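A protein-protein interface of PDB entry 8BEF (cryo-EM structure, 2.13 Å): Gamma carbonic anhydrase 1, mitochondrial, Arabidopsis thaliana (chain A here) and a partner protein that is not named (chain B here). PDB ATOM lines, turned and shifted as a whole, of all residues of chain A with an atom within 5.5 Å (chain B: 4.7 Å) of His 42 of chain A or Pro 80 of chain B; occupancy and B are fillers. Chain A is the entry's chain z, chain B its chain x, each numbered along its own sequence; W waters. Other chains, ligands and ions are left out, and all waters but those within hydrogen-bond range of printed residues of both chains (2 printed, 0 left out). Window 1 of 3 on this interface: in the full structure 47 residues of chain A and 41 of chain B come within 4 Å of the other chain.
The backbone carbonyl oxygen of Ala 65 of chain A lies close to a ring nitrogen (NE2) of His 42 of chain A (3.3 Å). The backbone NH (N) of His 42 of chain A lies within hydrogen-bond range of the side-chain hydroxyl (OG) of Ser 40 of chain A (3.2 Å). NE2 of His 42 of chain A lies within hydrogen-bond range of O of Pro 63 of chain A, at 2.9 Å. The side-chain amide nitrogen (NE2) of Gln 61 of chain B sits at hydrogen-bond distance from the backbone carbonyl oxygen (O) of Pro 80 of chain B, 3.3 Å away.
Of the 8 printed residues of chain B, 3 touch a printed residue of chain A. Of the 9 printed residues of chain A, 4 touch a printed residue of chain B.
Among the printed residues, merely in contact across the chains: Arg 41 of chain A with Pro 80 of chain B (3.6 Å), His 42 of chain A with Pro 80 of chain B (3.6 Å), Arg 43 of chain A with Phe 235 of chain B (3.6 Å) and Ser 66 of chain A with Asn 81 of chain B (3.6 Å).
Water W1 bridges O of Ser 64 of chain A (2.6 Å) and ND2 of Asn 81 of chain B (3.2 Å). Water W2 lies within hydrogen-bond range of O of Pro 80 of chain B (2.8 Å) and N of Arg 41 of chain A (3.0 Å).
Of the printed residues of chain B, Arg 41 of chain A touches Pro 80 (3.6 Å). Of chain B, only Pro 80 comes within 4 Å of His 42 of chain A. Tyr 77 of chain B touches none of the printed residues of chain A. Of chain A, only Arg 41 (3.6 Å) and His 42 (3.6 Å) come within 4 Å of Pro 80 of chain B. Of the printed residues of chain A, Asn 81 of chain B touches Ser 66. The nearest residue of chain B that does not touch His 42 of chain A is Asn 81 of chain B (4.1 Å). The nearest residue of chain A that does not touch Pro 80 of chain B is Ser 40 of chain A (4.8 Å). The nearest printed residue of chain A that does not touch Asn 81 of chain B is His 42 of chain A (4.1 Å).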
ATOM      1  N   SER A  40       4.224  -3.408  20.217  1.00  0.00           N
ATOM      2  CA  SER A  40       3.395  -2.212  20.244  1.00  0.00           C
ATOM      3  C   SER A  40       2.185  -2.411  21.148  1.00  0.00           C
ATOM      4  O   SER A  40       1.490  -3.426  21.067  1.00  0.00           O
ATOM      5  CB  SER A  40       2.940  -1.849  18.835  1.00  0.00           C
ATOM      6  OG  SER A  40       1.984  -0.805  18.872  1.00  0.00           O
ATOM      7  N   ARG A  41       1.931  -1.426  22.000  1.00  0.00           N
ATOM      8  CA  ARG A  41       0.778  -1.432  22.884  1.00  0.00           C
ATOM      9  C   ARG A  41      -0.378  -0.616  22.324  1.00  0.00           C
ATOM     10  O   ARG A  41      -1.323  -0.309  23.054  1.00  0.00           O
ATOM     11  CB  ARG A  41       1.187  -0.930  24.269  1.00  0.00           C
ATOM     12  CG  ARG A  41       2.481  -1.573  24.759  1.00  0.00           C
ATOM     13  CD  ARG A  41       2.726  -1.362  26.242  1.00  0.00           C
ATOM     14  NE  ARG A  41       1.664  -1.912  27.076  1.00  0.00           N
ATOM     15  CZ  ARG A  41       1.723  -1.993  28.400  1.00  0.00           C
ATOM     16  NH1 ARG A  41       2.787  -1.581  29.069  1.00  0.00           N
ATOM     17  NH2 ARG A  41       0.688  -2.493  29.068  1.00  0.00           N
ATOM     18  N   HIS A  42      -0.312  -0.252  21.046  1.00  0.00           N
ATOM     19  CA  HIS A  42      -1.398   0.477  20.413  1.00  0.00           C
ATOM     20  C   HIS A  42      -2.668  -0.360  20.398  1.00  0.00           C
ATOM     21  O   HIS A  42      -2.647  -1.539  20.043  1.00  0.00           O
ATOM     22  CB  HIS A  42      -1.020   0.862  18.984  1.00  0.00           C
ATOM     23  CG  HIS A  42      -2.187   1.306  18.159  1.00  0.00           C
ATOM     24  ND1 HIS A  42      -2.796   2.529  18.334  1.00  0.00           N
ATOM     25  CD2 HIS A  42      -2.867   0.686  17.166  1.00  0.00           C
ATOM     26  CE1 HIS A  42      -3.795   2.648  17.478  1.00  0.00           C
ATOM     27  NE2 HIS A  42      -3.860   1.543  16.758  1.00  0.00           N
ATOM     28  N   ARG A  43      -3.776   0.262  20.779  1.00  0.00           N
ATOM     29  CA  ARG A  43      -5.095  -0.342  20.688  1.00  0.00           C
ATOM     30  C   ARG A  43      -5.947   0.510  19.760  1.00  0.00           C
ATOM     31  O   ARG A  43      -6.049   1.726  19.952  1.00  0.00           O
ATOM     32  CB  ARG A  43      -5.745  -0.457  22.072  1.00  0.00           C
ATOM     33  CG  ARG A  43      -5.261  -1.655  22.883  1.00  0.00           C
ATOM     34  CD  ARG A  43      -5.811  -1.641  24.302  1.00  0.00           C
ATOM     35  NE  ARG A  43      -5.291  -0.525  25.080  1.00  0.00           N
ATOM     36  CZ  ARG A  43      -5.832  -0.067  26.200  1.00  0.00           C
ATOM     37  NH1 ARG A  43      -6.915  -0.620  26.724  1.00  0.00           N
ATOM     38  NH2 ARG A  43      -5.265   0.963  26.820  1.00  0.00           N
ATOM     39  N   THR A  44      -6.539  -0.123  18.749  1.00  0.00           N
ATOM     40  CA  THR A  44      -7.405   0.610  17.832  1.00  0.00           C
ATOM     41  C   THR A  44      -8.588   1.219  18.572  1.00  0.00           C
ATOM     42  O   THR A  44      -8.948   2.378  18.339  1.00  0.00           O
ATOM     43  CB  THR A  44      -7.883  -0.315  16.712  1.00  0.00           C
ATOM     44  OG1 THR A  44      -6.753  -0.927  16.080  1.00  0.00           O
ATOM     45  CG2 THR A  44      -8.673   0.461  15.680  1.00  0.00           C
ATOM     46  N   PRO A  63      -6.665  -0.295  11.236  1.00  0.00           N
ATOM     47  CA  PRO A  63      -6.005  -0.755  12.473  1.00  0.00           C
ATOM     48  C   PRO A  63      -5.143   0.304  13.135  1.00  0.00           C
ATOM     49  O   PRO A  63      -5.080   0.361  14.369  1.00  0.00           O
ATOM     50  CB  PRO A  63      -5.169  -1.953  11.995  1.00  0.00           C
ATOM     51  CG  PRO A  63      -5.827  -2.408  10.736  1.00  0.00           C
ATOM     52  CD  PRO A  63      -6.402  -1.183  10.091  1.00  0.00           C
ATOM     53  N   SER A  64      -4.484   1.154  12.349  1.00  0.00           N
ATOM     54  CA  SER A  64      -3.608   2.185  12.890  1.00  0.00           C
ATOM     55  C   SER A  64      -4.365   3.383  13.457  1.00  0.00           C
ATOM     56  O   SER A  64      -3.737   4.257  14.061  1.00  0.00           O
ATOM     57  CB  SER A  64      -2.626   2.656  11.811  1.00  0.00           C
ATOM     58  OG  SER A  64      -3.302   3.295  10.741  1.00  0.00           O
ATOM     59  N   ALA A  65      -5.681   3.452  13.276  1.00  0.00           N
ATOM     60  CA  ALA A  65      -6.454   4.548  13.841  1.00  0.00           C
ATOM     61  C   ALA A  65      -6.552   4.418  15.358  1.00  0.00           C
ATOM     62  O   ALA A  65      -6.489   3.321  15.915  1.00  0.00           O
ATOM     63  CB  ALA A  65      -7.852   4.587  13.229  1.00  0.00           C
ATOM     64  N   SER A  66      -6.702   5.558  16.027  1.00  0.00           N
ATOM     65  CA  SER A  66      -6.865   5.615  17.474  1.00  0.00           C
ATOM     66  C   SER A  66      -8.264   6.125  17.800  1.00  0.00           C
ATOM     67  O   SER A  66      -8.599   7.272  17.491  1.00  0.00           O
ATOM     68  CB  SER A  66      -5.808   6.515  18.117  1.00  0.00           C
ATOM     69  OG  SER A  66      -4.497   6.080  17.817  1.00  0.00           O
ATOM     70  N   GLN B  61       8.218   1.941  19.776  1.00  0.00           N
ATOM     71  CA  GLN B  61       8.047   3.302  20.271  1.00  0.00           C
ATOM     72  C   GLN B  61       9.388   4.004  20.458  1.00  0.00           C
ATOM     73  O   GLN B  61       9.518   5.197  20.156  1.00  0.00           O
ATOM     74  CB  GLN B  61       7.263   3.288  21.583  1.00  0.00           C
ATOM     75  CG  GLN B  61       7.012   4.664  22.165  1.00  0.00           C
ATOM     76  CD  GLN B  61       6.253   4.620  23.477  1.00  0.00           C
ATOM     77  OE1 GLN B  61       6.832   4.384  24.533  1.00  0.00           O
ATOM     78  NE2 GLN B  61       4.950   4.854  23.413  1.00  0.00           N
ATOM     79  N   TYR B  77       3.801  10.569  30.562  1.00  0.00           N
ATOM     80  CA  TYR B  77       2.930   9.758  29.722  1.00  0.00           C
ATOM     81  C   TYR B  77       3.353   9.898  28.265  1.00  0.00           C
ATOM     82  O   TYR B  77       3.390  11.007  27.729  1.00  0.00           O
ATOM     83  CB  TYR B  77       1.463  10.157  29.871  1.00  0.00           C
ATOM     84  CG  TYR B  77       0.572   9.411  28.906  1.00  0.00           C
ATOM     85  CD1 TYR B  77       0.408   8.038  29.011  1.00  0.00           C
ATOM     86  CD2 TYR B  77      -0.079  10.071  27.869  1.00  0.00           C
ATOM     87  CE1 TYR B  77      -0.391   7.343  28.129  1.00  0.00           C
ATOM     88  CE2 TYR B  77      -0.886   9.379  26.978  1.00  0.00           C
ATOM     89  CZ  TYR B  77      -1.032   8.014  27.115  1.00  0.00           C
ATOM     90  OH  TYR B  77      -1.824   7.308  26.242  1.00  0.00           O
ATOM     91  N   VAL B  78       3.657   8.775  27.627  1.00  0.00           N
ATOM     92  CA  VAL B  78       3.916   8.729  26.194  1.00  0.00           C
ATOM     93  C   VAL B  78       2.937   7.736  25.584  1.00  0.00           C
ATOM     94  O   VAL B  78       2.936   6.555  25.952  1.00  0.00           O
ATOM     95  CB  VAL B  78       5.371   8.345  25.881  1.00  0.00           C
ATOM     96  CG1 VAL B  78       5.586   8.276  24.379  1.00  0.00           C
ATOM     97  CG2 VAL B  78       6.330   9.343  26.518  1.00  0.00           C
ATOM     98  N   ALA B  79       2.112   8.213  24.655  1.00  0.00           N
ATOM     99  CA  ALA B  79       1.086   7.375  24.057  1.00  0.00           C
ATOM    100  C   ALA B  79       1.728   6.189  23.335  1.00  0.00           C
ATOM    101  O   ALA B  79       2.853   6.289  22.840  1.00  0.00           O
ATOM    102  CB  ALA B  79       0.231   8.186  23.085  1.00  0.00           C
ATOM    103  N   PRO B  80       1.035   5.047  23.277  1.00  0.00           N
ATOM    104  CA  PRO B  80       1.666   3.831  22.729  1.00  0.00           C
ATOM    105  C   PRO B  80       2.167   3.963  21.298  1.00  0.00           C
ATOM    106  O   PRO B  80       3.203   3.376  20.968  1.00  0.00           O
ATOM    107  CB  PRO B  80       0.548   2.784  22.841  1.00  0.00           C
ATOM    108  CG  PRO B  80      -0.328   3.288  23.929  1.00  0.00           C
ATOM    109  CD  PRO B  80      -0.318   4.777  23.795  1.00  0.00           C
ATOM    110  N   ASN B  81       1.480   4.712  20.436  1.00  0.00           N
ATOM    111  CA  ASN B  81       1.864   4.780  19.031  1.00  0.00           C
ATOM    112  C   ASN B  81       2.775   5.964  18.712  1.00  0.00           C
ATOM    113  O   ASN B  81       3.061   6.210  17.538  1.00  0.00           O
ATOM    114  CB  ASN B  81       0.619   4.800  18.135  1.00  0.00           C
ATOM    115  CG  ASN B  81      -0.177   6.085  18.250  1.00  0.00           C
ATOM    116  OD1 ASN B  81      -0.085   6.806  19.239  1.00  0.00           O
ATOM    117  ND2 ASN B  81      -0.987   6.361  17.239  1.00  0.00           N
ATOM    118  N   VAL B  82       3.235   6.695  19.730  1.00  0.00           N
ATOM    119  CA  VAL B  82       4.230   7.739  19.528  1.00  0.00           C
ATOM    120  C   VAL B  82       5.561   7.109  19.121  1.00  0.00           C
ATOM    121  O   VAL B  82       5.902   5.997  19.544  1.00  0.00           O
ATOM    122  CB  VAL B  82       4.378   8.579  20.813  1.00  0.00           C
ATOM    123  CG1 VAL B  82       5.585   9.509  20.741  1.00  0.00           C
ATOM    124  CG2 VAL B  82       3.108   9.365  21.087  1.00  0.00           C
ATOM    125  N   PHE B 235      -2.099   1.614  31.894  1.00  0.00           N
ATOM    126  CA  PHE B 235      -1.066   0.724  31.377  1.00  0.00           C
ATOM    127  C   PHE B 235      -0.246   0.159  32.527  1.00  0.00           C
ATOM    128  O   PHE B 235       0.355   0.914  33.296  1.00  0.00           O
ATOM    129  CB  PHE B 235      -0.159   1.459  30.387  1.00  0.00           C
ATOM    130  CG  PHE B 235      -0.860   1.900  29.139  1.00  0.00           C
ATOM    131  CD1 PHE B 235      -0.995   1.038  28.063  1.00  0.00           C
ATOM    132  CD2 PHE B 235      -1.395   3.175  29.042  1.00  0.00           C
ATOM    133  CE1 PHE B 235      -1.642   1.440  26.914  1.00  0.00           C
ATOM    134  CE2 PHE B 235      -2.047   3.582  27.897  1.00  0.00           C
ATOM    135  CZ  PHE B 235      -2.169   2.713  26.830  1.00  0.00           C
HETATM  136  O   HOH W   1      -1.482   3.839  15.309  1.00  0.00           O
HETATM  137  O   HOH W   2       3.718   0.941  22.347  1.00  0.00           O
